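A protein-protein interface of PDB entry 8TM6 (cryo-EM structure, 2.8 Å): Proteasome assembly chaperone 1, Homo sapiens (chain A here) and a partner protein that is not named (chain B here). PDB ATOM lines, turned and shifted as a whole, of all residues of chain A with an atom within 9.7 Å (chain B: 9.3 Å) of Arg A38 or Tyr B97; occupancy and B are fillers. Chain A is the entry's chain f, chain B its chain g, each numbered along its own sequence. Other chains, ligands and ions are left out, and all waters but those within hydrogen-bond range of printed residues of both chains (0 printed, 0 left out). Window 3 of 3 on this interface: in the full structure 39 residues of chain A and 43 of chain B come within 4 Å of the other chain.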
ATOM      1  N   GLY A  17      21.359  18.744  -3.450  1.00  0.00           N
ATOM      2  CA  GLY A  17      20.230  18.665  -2.548  1.00  0.00           C
ATOM      3  C   GLY A  17      19.773  19.995  -2.004  1.00  0.00           C
ATOM      4  O   GLY A  17      19.206  20.047  -0.910  1.00  0.00           O
ATOM      5  N   ASP A  20      15.807  20.572  -1.159  1.00  0.00           N
ATOM      6  CA  ASP A  20      15.275  20.098   0.115  1.00  0.00           C
ATOM      7  C   ASP A  20      15.345  21.195   1.170  1.00  0.00           C
ATOM      8  O   ASP A  20      14.355  21.484   1.852  1.00  0.00           O
ATOM      9  CB  ASP A  20      16.043  18.858   0.573  1.00  0.00           C
ATOM     10  CG  ASP A  20      15.942  17.712  -0.415  1.00  0.00           C
ATOM     11  OD1 ASP A  20      15.046  17.751  -1.284  1.00  0.00           O
ATOM     12  OD2 ASP A  20      16.759  16.773  -0.321  1.00  0.00           O
ATOM     13  N   GLU A  21      16.512  21.829   1.309  1.00  0.00           N
ATOM     14  CA  GLU A  21      16.649  22.923   2.264  1.00  0.00           C
ATOM     15  C   GLU A  21      15.774  24.106   1.872  1.00  0.00           C
ATOM     16  O   GLU A  21      15.153  24.740   2.735  1.00  0.00           O
ATOM     17  CB  GLU A  21      18.115  23.347   2.366  1.00  0.00           C
ATOM     18  CG  GLU A  21      18.358  24.594   3.211  1.00  0.00           C
ATOM     19  CD  GLU A  21      18.139  25.887   2.446  1.00  0.00           C
ATOM     20  OE1 GLU A  21      17.561  26.831   3.024  1.00  0.00           O
ATOM     21  OE2 GLU A  21      18.541  25.956   1.265  1.00  0.00           O
ATOM     22  N   GLU A  22      15.713  24.423   0.576  1.00  0.00           N
ATOM     23  CA  GLU A  22      14.928  25.570   0.135  1.00  0.00           C
ATOM     24  C   GLU A  22      13.469  25.416   0.536  1.00  0.00           C
ATOM     25  O   GLU A  22      12.846  26.367   1.022  1.00  0.00           O
ATOM     26  CB  GLU A  22      15.055  25.749  -1.380  1.00  0.00           C
ATOM     27  CG  GLU A  22      16.488  25.873  -1.872  1.00  0.00           C
ATOM     28  CD  GLU A  22      17.051  27.267  -1.688  1.00  0.00           C
ATOM     29  OE1 GLU A  22      16.591  27.981  -0.773  1.00  0.00           O
ATOM     30  OE2 GLU A  22      17.969  27.642  -2.446  1.00  0.00           O
ATOM     31  N   GLU A  23      12.904  24.224   0.341  1.00  0.00           N
ATOM     32  CA  GLU A  23      11.572  23.961   0.871  1.00  0.00           C
ATOM     33  C   GLU A  23      11.560  24.040   2.392  1.00  0.00           C
ATOM     34  O   GLU A  23      10.662  24.653   2.980  1.00  0.00           O
ATOM     35  CB  GLU A  23      11.072  22.592   0.410  1.00  0.00           C
ATOM     36  CG  GLU A  23      10.091  21.934   1.380  1.00  0.00           C
ATOM     37  CD  GLU A  23       8.838  22.767   1.621  1.00  0.00           C
ATOM     38  OE1 GLU A  23       8.765  23.907   1.115  1.00  0.00           O
ATOM     39  OE2 GLU A  23       7.935  22.288   2.336  1.00  0.00           O
ATOM     40  N   GLU A  24      12.547  23.420   3.045  1.00  0.00           N
ATOM     41  CA  GLU A  24      12.543  23.348   4.502  1.00  0.00           C
ATOM     42  C   GLU A  24      12.447  24.738   5.117  1.00  0.00           C
ATOM     43  O   GLU A  24      11.795  24.924   6.152  1.00  0.00           O
ATOM     44  CB  GLU A  24      13.798  22.612   4.981  1.00  0.00           C
ATOM     45  CG  GLU A  24      14.250  22.914   6.408  1.00  0.00           C
ATOM     46  CD  GLU A  24      15.666  22.441   6.674  1.00  0.00           C
ATOM     47  OE1 GLU A  24      16.146  21.556   5.935  1.00  0.00           O
ATOM     48  OE2 GLU A  24      16.298  22.954   7.621  1.00  0.00           O
ATOM     49  N   GLU A  25      13.088  25.723   4.497  1.00  0.00           N
ATOM     50  CA  GLU A  25      13.055  27.094   4.991  1.00  0.00           C
ATOM     51  C   GLU A  25      12.262  27.985   4.042  1.00  0.00           C
ATOM     52  O   GLU A  25      11.227  27.577   3.513  1.00  0.00           O
ATOM     53  CB  GLU A  25      14.476  27.638   5.159  1.00  0.00           C
ATOM     54  CG  GLU A  25      15.441  26.682   5.856  1.00  0.00           C
ATOM     55  CD  GLU A  25      15.053  26.382   7.294  1.00  0.00           C
ATOM     56  OE1 GLU A  25      15.847  25.722   7.995  1.00  0.00           O
ATOM     57  OE2 GLU A  25      13.962  26.810   7.726  1.00  0.00           O
ATOM     58  N   GLU A  30       8.192  27.755  14.550  1.00  0.00           N
ATOM     59  CA  GLU A  30       7.268  27.067  13.656  1.00  0.00           C
ATOM     60  C   GLU A  30       6.046  26.571  14.421  1.00  0.00           C
ATOM     61  O   GLU A  30       5.887  26.852  15.609  1.00  0.00           O
ATOM     62  CB  GLU A  30       7.966  25.896  12.962  1.00  0.00           C
ATOM     63  N   THR A  31       5.182  25.834  13.732  1.00  0.00           N
ATOM     64  CA  THR A  31       3.986  25.305  14.369  1.00  0.00           C
ATOM     65  C   THR A  31       4.381  24.322  15.468  1.00  0.00           C
ATOM     66  O   THR A  31       5.269  23.485  15.252  1.00  0.00           O
ATOM     67  CB  THR A  31       3.090  24.612  13.342  1.00  0.00           C
ATOM     68  N   PRO A  32       3.760  24.384  16.649  1.00  0.00           N
ATOM     69  CA  PRO A  32       4.174  23.469  17.726  1.00  0.00           C
ATOM     70  C   PRO A  32       3.962  22.004  17.389  1.00  0.00           C
ATOM     71  O   PRO A  32       4.771  21.164  17.798  1.00  0.00           O
ATOM     72  CB  PRO A  32       3.319  23.906  18.926  1.00  0.00           C
ATOM     73  CG  PRO A  32       2.292  24.854  18.407  1.00  0.00           C
ATOM     74  CD  PRO A  32       2.495  25.077  16.947  1.00  0.00           C
ATOM     75  N   GLU A  33       2.898  21.668  16.657  1.00  0.00           N
ATOM     76  CA  GLU A  33       2.661  20.276  16.288  1.00  0.00           C
ATOM     77  C   GLU A  33       3.753  19.768  15.354  1.00  0.00           C
ATOM     78  O   GLU A  33       4.245  18.642  15.499  1.00  0.00           O
ATOM     79  CB  GLU A  33       1.283  20.139  15.638  1.00  0.00           C
ATOM     80  N   ASP A  34       4.138  20.590  14.375  1.00  0.00           N
ATOM     81  CA  ASP A  34       5.199  20.196  13.457  1.00  0.00           C
ATOM     82  C   ASP A  34       6.510  19.994  14.203  1.00  0.00           C
ATOM     83  O   ASP A  34       7.242  19.031  13.951  1.00  0.00           O
ATOM     84  CB  ASP A  34       5.357  21.246  12.356  1.00  0.00           C
ATOM     85  CG  ASP A  34       6.216  20.760  11.204  1.00  0.00           C
ATOM     86  OD1 ASP A  34       6.307  19.531  11.004  1.00  0.00           O
ATOM     87  OD2 ASP A  34       6.800  21.608  10.497  1.00  0.00           O
ATOM     88  N   ARG A  35       6.820  20.894  15.139  1.00  0.00           N
ATOM     89  CA  ARG A  35       8.031  20.746  15.937  1.00  0.00           C
ATOM     90  C   ARG A  35       7.983  19.472  16.772  1.00  0.00           C
ATOM     91  O   ARG A  35       8.980  18.753  16.892  1.00  0.00           O
ATOM     92  CB  ARG A  35       8.216  21.971  16.834  1.00  0.00           C
ATOM     93  N   GLU A  36       6.823  19.181  17.366  1.00  0.00           N
ATOM     94  CA  GLU A  36       6.699  17.985  18.193  1.00  0.00           C
ATOM     95  C   GLU A  36       6.905  16.720  17.371  1.00  0.00           C
ATOM     96  O   GLU A  36       7.634  15.813  17.791  1.00  0.00           O
ATOM     97  CB  GLU A  36       5.332  17.962  18.875  1.00  0.00           C
ATOM     98  N   VAL A  37       6.278  16.636  16.195  1.00  0.00           N
ATOM     99  CA  VAL A  37       6.458  15.446  15.366  1.00  0.00           C
ATOM    100  C   VAL A  37       7.887  15.361  14.842  1.00  0.00           C
ATOM    101  O   VAL A  37       8.442  14.262  14.711  1.00  0.00           O
ATOM    102  CB  VAL A  37       5.426  15.412  14.221  1.00  0.00           C
ATOM    103  CG1 VAL A  37       4.011  15.492  14.779  1.00  0.00           C
ATOM    104  CG2 VAL A  37       5.670  16.539  13.235  1.00  0.00           C
ATOM    105  N   ARG A  38       8.511  16.502  14.535  1.00  0.00           N
ATOM    106  CA  ARG A  38       9.902  16.479  14.099  1.00  0.00           C
ATOM    107  C   ARG A  38      10.813  15.954  15.201  1.00  0.00           C
ATOM    108  O   ARG A  38      11.725  15.162  14.939  1.00  0.00           O
ATOM    109  CB  ARG A  38      10.332  17.880  13.662  1.00  0.00           C
ATOM    110  CG  ARG A  38      11.784  17.982  13.212  1.00  0.00           C
ATOM    111  CD  ARG A  38      12.163  19.414  12.867  1.00  0.00           C
ATOM    112  NE  ARG A  38      11.817  20.350  13.930  1.00  0.00           N
ATOM    113  CZ  ARG A  38      12.623  20.692  14.926  1.00  0.00           C
ATOM    114  NH1 ARG A  38      13.840  20.186  15.040  1.00  0.00           N
ATOM    115  NH2 ARG A  38      12.196  21.564  15.834  1.00  0.00           N
ATOM    116  N   LEU A  39      10.584  16.384  16.444  1.00  0.00           N
ATOM    117  CA  LEU A  39      11.379  15.874  17.557  1.00  0.00           C
ATOM    118  C   LEU A  39      11.109  14.392  17.793  1.00  0.00           C
ATOM    119  O   LEU A  39      12.023  13.637  18.145  1.00  0.00           O
ATOM    120  CB  LEU A  39      11.091  16.682  18.822  1.00  0.00           C
ATOM    121  CG  LEU A  39      11.492  18.159  18.768  1.00  0.00           C
ATOM    122  CD1 LEU A  39      11.004  18.889  20.008  1.00  0.00           C
ATOM    123  CD2 LEU A  39      12.998  18.307  18.616  1.00  0.00           C
ATOM    124  N   GLN A  40       9.859  13.962  17.611  1.00  0.00           N
ATOM    125  CA  GLN A  40       9.553  12.539  17.715  1.00  0.00           C
ATOM    126  C   GLN A  40      10.339  11.739  16.684  1.00  0.00           C
ATOM    127  O   GLN A  40      10.919  10.695  17.004  1.00  0.00           O
ATOM    128  CB  GLN A  40       8.052  12.312  17.534  1.00  0.00           C
ATOM    129  CG  GLN A  40       7.279  12.189  18.839  1.00  0.00           C
ATOM    130  CD  GLN A  40       7.265  10.772  19.383  1.00  0.00           C
ATOM    131  OE1 GLN A  40       7.673   9.828  18.704  1.00  0.00           O
ATOM    132  NE2 GLN A  40       6.793  10.616  20.613  1.00  0.00           N
ATOM    133  N   LEU A  41      10.382  12.225  15.443  1.00  0.00           N
ATOM    134  CA  LEU A  41      11.175  11.554  14.416  1.00  0.00           C
ATOM    135  C   LEU A  41      12.656  11.566  14.773  1.00  0.00           C
ATOM    136  O   LEU A  41      13.360  10.569  14.572  1.00  0.00           O
ATOM    137  CB  LEU A  41      10.946  12.221  13.059  1.00  0.00           C
ATOM    138  CG  LEU A  41      11.552  11.516  11.843  1.00  0.00           C
ATOM    139  CD1 LEU A  41      11.082  10.072  11.742  1.00  0.00           C
ATOM    140  CD2 LEU A  41      11.220  12.278  10.570  1.00  0.00           C
ATOM    141  N   ALA A  42      13.149  12.689  15.298  1.00  0.00           N
ATOM    142  CA  ALA A  42      14.561  12.783  15.651  1.00  0.00           C
ATOM    143  C   ALA A  42      14.932  11.763  16.719  1.00  0.00           C
ATOM    144  O   ALA A  42      15.965  11.091  16.615  1.00  0.00           O
ATOM    145  CB  ALA A  42      14.887  14.198  16.129  1.00  0.00           C
ATOM    146  N   ARG A  43      14.103  11.631  17.756  1.00  0.00           N
ATOM    147  CA  ARG A  43      14.370  10.645  18.796  1.00  0.00           C
ATOM    148  C   ARG A  43      14.113   9.220  18.324  1.00  0.00           C
ATOM    149  O   ARG A  43      14.680   8.281  18.895  1.00  0.00           O
ATOM    150  CB  ARG A  43      13.529  10.936  20.042  1.00  0.00           C
ATOM    151  CG  ARG A  43      12.032  10.799  19.839  1.00  0.00           C
ATOM    152  CD  ARG A  43      11.264  11.289  21.056  1.00  0.00           C
ATOM    153  NE  ARG A  43      11.362  12.736  21.219  1.00  0.00           N
ATOM    154  CZ  ARG A  43      10.386  13.517  21.665  1.00  0.00           C
ATOM    155  NH1 ARG A  43       9.212  13.024  22.027  1.00  0.00           N
ATOM    156  NH2 ARG A  43      10.595  14.827  21.756  1.00  0.00           N
ATOM    157  N   LYS A  44      13.276   9.036  17.302  1.00  0.00           N
ATOM    158  CA  LYS A  44      13.088   7.713  16.719  1.00  0.00           C
ATOM    159  C   LYS A  44      14.287   7.286  15.883  1.00  0.00           C
ATOM    160  O   LYS A  44      14.606   6.094  15.828  1.00  0.00           O
ATOM    161  CB  LYS A  44      11.822   7.702  15.861  1.00  0.00           C
ATOM    162  CG  LYS A  44      11.440   6.337  15.313  1.00  0.00           C
ATOM    163  CD  LYS A  44      10.229   6.438  14.398  1.00  0.00           C
ATOM    164  CE  LYS A  44       9.787   5.073  13.899  1.00  0.00           C
ATOM    165  NZ  LYS A  44       8.691   5.175  12.898  1.00  0.00           N
ATOM    166  N   ARG A  45      14.954   8.238  15.229  1.00  0.00           N
ATOM    167  CA  ARG A  45      16.074   7.931  14.350  1.00  0.00           C
ATOM    168  C   ARG A  45      17.412   7.866  15.075  1.00  0.00           C
ATOM    169  O   ARG A  45      18.375   7.333  14.513  1.00  0.00           O
ATOM    170  CB  ARG A  45      16.165   8.980  13.237  1.00  0.00           C
ATOM    171  CG  ARG A  45      15.004   8.952  12.256  1.00  0.00           C
ATOM    172  CD  ARG A  45      15.252   9.884  11.081  1.00  0.00           C
ATOM    173  NE  ARG A  45      16.279   9.376  10.180  1.00  0.00           N
ATOM    174  CZ  ARG A  45      16.046   8.588   9.138  1.00  0.00           C
ATOM    175  NH1 ARG A  45      14.822   8.186   8.832  1.00  0.00           N
ATOM    176  NH2 ARG A  45      17.067   8.190   8.385  1.00  0.00           N
ATOM    177  N   GLU A  46      17.499   8.389  16.294  1.00  0.00           N
ATOM    178  CA  GLU A  46      18.780   8.459  16.983  1.00  0.00           C
ATOM    179  C   GLU A  46      19.276   7.067  17.362  1.00  0.00           C
ATOM    180  O   GLU A  46      18.493   6.160  17.658  1.00  0.00           O
ATOM    181  CB  GLU A  46      18.670   9.328  18.236  1.00  0.00           C
ATOM    182  CG  GLU A  46      18.095   8.608  19.444  1.00  0.00           C
ATOM    183  CD  GLU A  46      17.536   9.560  20.485  1.00  0.00           C
ATOM    184  OE1 GLU A  46      17.181   9.093  21.587  1.00  0.00           O
ATOM    185  OE2 GLU A  46      17.455  10.775  20.205  1.00  0.00           O
ATOM    186  N   ASP A 144      22.624  11.044   8.618  1.00  0.00           N
ATOM    187  CA  ASP A 144      22.572  11.881   9.810  1.00  0.00           C
ATOM    188  C   ASP A 144      22.922  11.129  11.087  1.00  0.00           C
ATOM    189  O   ASP A 144      22.920  11.741  12.159  1.00  0.00           O
ATOM    190  CB  ASP A 144      21.178  12.494   9.960  1.00  0.00           C
ATOM    191  CG  ASP A 144      20.086  11.446  10.043  1.00  0.00           C
ATOM    192  OD1 ASP A 144      20.198  10.415   9.349  1.00  0.00           O
ATOM    193  OD2 ASP A 144      19.118  11.654  10.805  1.00  0.00           O
ATOM    194  N   ASP B  50      29.507  17.953  12.232  1.00  0.00           N
ATOM    195  CA  ASP B  50      28.422  16.998  12.027  1.00  0.00           C
ATOM    196  C   ASP B  50      27.554  17.381  10.836  1.00  0.00           C
ATOM    197  O   ASP B  50      26.770  16.558  10.350  1.00  0.00           O
ATOM    198  CB  ASP B  50      27.550  16.888  13.282  1.00  0.00           C
ATOM    199  CG  ASP B  50      27.387  18.214  14.006  1.00  0.00           C
ATOM    200  OD1 ASP B  50      27.735  19.260  13.420  1.00  0.00           O
ATOM    201  OD2 ASP B  50      26.909  18.207  15.160  1.00  0.00           O
ATOM    202  N   CYS B  51      27.678  18.619  10.355  1.00  0.00           N
ATOM    203  CA  CYS B  51      26.753  19.124   9.345  1.00  0.00           C
ATOM    204  C   CYS B  51      27.067  18.570   7.961  1.00  0.00           C
ATOM    205  O   CYS B  51      26.152  18.306   7.172  1.00  0.00           O
ATOM    206  CB  CYS B  51      26.792  20.649   9.348  1.00  0.00           C
ATOM    207  SG  CYS B  51      27.060  21.319  11.005  1.00  0.00           S
ATOM    208  N   PHE B  94      25.109  18.730   2.610  1.00  0.00           N
ATOM    209  CA  PHE B  94      24.620  19.062   3.938  1.00  0.00           C
ATOM    210  C   PHE B  94      23.509  18.105   4.360  1.00  0.00           C
ATOM    211  O   PHE B  94      22.937  17.372   3.550  1.00  0.00           O
ATOM    212  CB  PHE B  94      24.114  20.507   3.971  1.00  0.00           C
ATOM    213  CG  PHE B  94      25.146  21.495   4.420  1.00  0.00           C
ATOM    214  CD1 PHE B  94      26.082  21.986   3.528  1.00  0.00           C
ATOM    215  CD2 PHE B  94      25.183  21.932   5.732  1.00  0.00           C
ATOM    216  CE1 PHE B  94      27.034  22.895   3.934  1.00  0.00           C
ATOM    217  CE2 PHE B  94      26.136  22.842   6.143  1.00  0.00           C
ATOM    218  CZ  PHE B  94      27.061  23.323   5.241  1.00  0.00           C
ATOM    219  N   ILE B  95      23.209  18.125   5.655  1.00  0.00           N
ATOM    220  CA  ILE B  95      22.116  17.351   6.232  1.00  0.00           C
ATOM    221  C   ILE B  95      20.990  18.311   6.588  1.00  0.00           C
ATOM    222  O   ILE B  95      21.211  19.509   6.803  1.00  0.00           O
ATOM    223  CB  ILE B  95      22.588  16.550   7.465  1.00  0.00           C
ATOM    224  CG1 ILE B  95      23.913  15.849   7.155  1.00  0.00           C
ATOM    225  CG2 ILE B  95      21.526  15.539   7.891  1.00  0.00           C
ATOM    226  CD1 ILE B  95      24.274  14.730   8.108  1.00  0.00           C
ATOM    227  N   LYS B  96      19.768  17.788   6.635  1.00  0.00           N
ATOM    228  CA  LYS B  96      18.616  18.626   6.933  1.00  0.00           C
ATOM    229  C   LYS B  96      18.751  19.254   8.315  1.00  0.00           C
ATOM    230  O   LYS B  96      19.176  18.604   9.275  1.00  0.00           O
ATOM    231  CB  LYS B  96      17.328  17.805   6.847  1.00  0.00           C
ATOM    232  CG  LYS B  96      16.092  18.639   6.555  1.00  0.00           C
ATOM    233  CD  LYS B  96      14.812  17.881   6.869  1.00  0.00           C
ATOM    234  CE  LYS B  96      13.615  18.503   6.165  1.00  0.00           C
ATOM    235  NZ  LYS B  96      13.472  18.019   4.764  1.00  0.00           N
ATOM    236  N   TYR B  97      18.385  20.532   8.409  1.00  0.00           N
ATOM    237  CA  TYR B  97      18.448  21.280   9.665  1.00  0.00           C
ATOM    238  C   TYR B  97      19.861  21.281  10.243  1.00  0.00           C
ATOM    239  O   TYR B  97      20.054  21.210  11.458  1.00  0.00           O
ATOM    240  CB  TYR B  97      17.449  20.727  10.683  1.00  0.00           C
ATOM    241  CG  TYR B  97      16.003  20.962  10.310  1.00  0.00           C
ATOM    242  CD1 TYR B  97      15.398  22.191  10.539  1.00  0.00           C
ATOM    243  CD2 TYR B  97      15.240  19.954   9.737  1.00  0.00           C
ATOM    244  CE1 TYR B  97      14.078  22.410  10.202  1.00  0.00           C
ATOM    245  CE2 TYR B  97      13.918  20.164   9.396  1.00  0.00           C
ATOM    246  CZ  TYR B  97      13.342  21.394   9.630  1.00  0.00           C
ATOM    247  OH  TYR B  97      12.025  21.610   9.293  1.00  0.00           O
ATOM    248  N   LYS B  98      20.862  21.370   9.363  1.00  0.00           N
ATOM    249  CA  LYS B  98      22.256  21.415   9.780  1.00  0.00           C
ATOM    250  C   LYS B  98      23.037  22.565   9.159  1.00  0.00           C
ATOM    251  O   LYS B  98      24.242  22.677   9.414  1.00  0.00           O
ATOM    252  CB  LYS B  98      22.959  20.090   9.442  1.00  0.00           C
ATOM    253  CG  LYS B  98      23.207  19.192  10.645  1.00  0.00           C
ATOM    254  CD  LYS B  98      21.936  18.497  11.099  1.00  0.00           C
ATOM    255  CE  LYS B  98      22.183  17.625  12.318  1.00  0.00           C
ATOM    256  NZ  LYS B  98      22.699  18.409  13.475  1.00  0.00           N
ATOM    257  N   SER B  99      22.398  23.420   8.359  1.00  0.00           N
ATOM    258  CA  SER B  99      23.110  24.542   7.755  1.00  0.00           C
ATOM    259  C   SER B  99      23.434  25.614   8.791  1.00  0.00           C
ATOM    260  O   SER B  99      24.551  26.143   8.823  1.00  0.00           O
ATOM    261  CB  SER B  99      22.282  25.130   6.614  1.00  0.00           C
ATOM    262  OG  SER B  99      22.033  24.159   5.613  1.00  0.00           O
ATOM    263  N   LYS B 100      22.463  25.955   9.637  1.00  0.00           N
ATOM    264  CA  LYS B 100      22.690  27.001  10.630  1.00  0.00           C
ATOM    265  C   LYS B 100      23.807  26.655  11.606  1.00  0.00           C
ATOM    266  O   LYS B 100      24.628  27.542  11.901  1.00  0.00           O
ATOM    267  CB  LYS B 100      21.388  27.290  11.388  1.00  0.00           C
ATOM    268  CG  LYS B 100      20.475  28.296  10.703  1.00  0.00           C
ATOM    269  CD  LYS B 100      19.630  27.637   9.624  1.00  0.00           C
ATOM    270  CE  LYS B 100      18.423  28.490   9.266  1.00  0.00           C
ATOM    271  NZ  LYS B 100      17.965  28.252   7.870  1.00  0.00           N
ATOM    272  N   PRO B 101      23.875  25.446  12.171  1.00  0.00           N
ATOM    273  CA  PRO B 101      25.034  25.112  13.014  1.00  0.00           C
ATOM    274  C   PRO B 101      26.358  25.264  12.292  1.00  0.00           C
ATOM    275  O   PRO B 101      27.329  25.753  12.883  1.00  0.00           O
ATOM    276  CB  PRO B 101      24.762  23.655  13.412  1.00  0.00           C
ATOM    277  CG  PRO B 101      23.285  23.520  13.351  1.00  0.00           C
ATOM    278  CD  PRO B 101      22.830  24.410  12.232  1.00  0.00           C
ATOM    279  N   PHE B 102      26.427  24.865  11.020  1.00  0.00           N
ATOM    280  CA  PHE B 102      27.672  25.015  10.274  1.00  0.00           C
ATOM    281  C   PHE B 102      28.028  26.484  10.107  1.00  0.00           C
ATOM    282  O   PHE B 102      29.193  26.870  10.251  1.00  0.00           O
ATOM    283  CB  PHE B 102      27.562  24.347   8.904  1.00  0.00           C
ATOM    284  CG  PHE B 102      28.792  24.508   8.058  1.00  0.00           C
ATOM    285  CD1 PHE B 102      29.883  23.674   8.235  1.00  0.00           C
ATOM    286  CD2 PHE B 102      28.867  25.506   7.102  1.00  0.00           C
ATOM    287  CE1 PHE B 102      31.017  23.822   7.462  1.00  0.00           C
ATOM    288  CE2 PHE B 102      29.999  25.659   6.327  1.00  0.00           C
ATOM    289  CZ  PHE B 102      31.077  24.817   6.508  1.00  0.00           C
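The guanidinium group (NE) of Arg A45 lies within salt-bridge range of the side-chain carboxylate (OD2) of Asp A144, at 3.7 Å. N of Ile B95 sits at hydrogen-bond distance from O of Cys B51 (3.3 Å).
Of chain B, only Tyr B97 comes within 4 Å of Arg A38. Of chain A, only Glu A24 (3.1 Å) and Arg A38 (3.96 Å) come within 4 Å of Tyr B97. No residue of chain B comes within 4 Å of Leu A39. No residue of chain A comes within 4 Å of Lys B98. Of the printed residues of chain B, Glu A24 touches Lys B96 (3.0 Å) and Tyr B97 (3.1 Å). Printed residues of chain A within 4 Å of Lys B100: Glu A25 (3.3 Å). The nearest residue of chain A that does not touch Tyr B97 is Glu A25 (4.4 Å).
Hydrophobic or aromatic side chains of chain B within 4 Å of the printed part of chain A: Ile B95 and Tyr B97. Among the printed residues, Asp or Glu carboxylates within 4 Å of a Lys or Arg side-chain nitrogen of the other chain: Glu A25 with Lys B100.
Glu A24 touches Lys B96 (OE1 to CG, 3.0 Å). CE2 of Tyr B97 touches CD of Arg A38, 3.96 Å away. Asp A144 touches Ile B95.
The side-chain carboxylate of Glu A24 sits close to the backbone NH of Tyr B97, 3.3 Å away. OE1 of Glu A25 is in salt-bridge range of NZ of Lys B100, at 3.3 Å.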
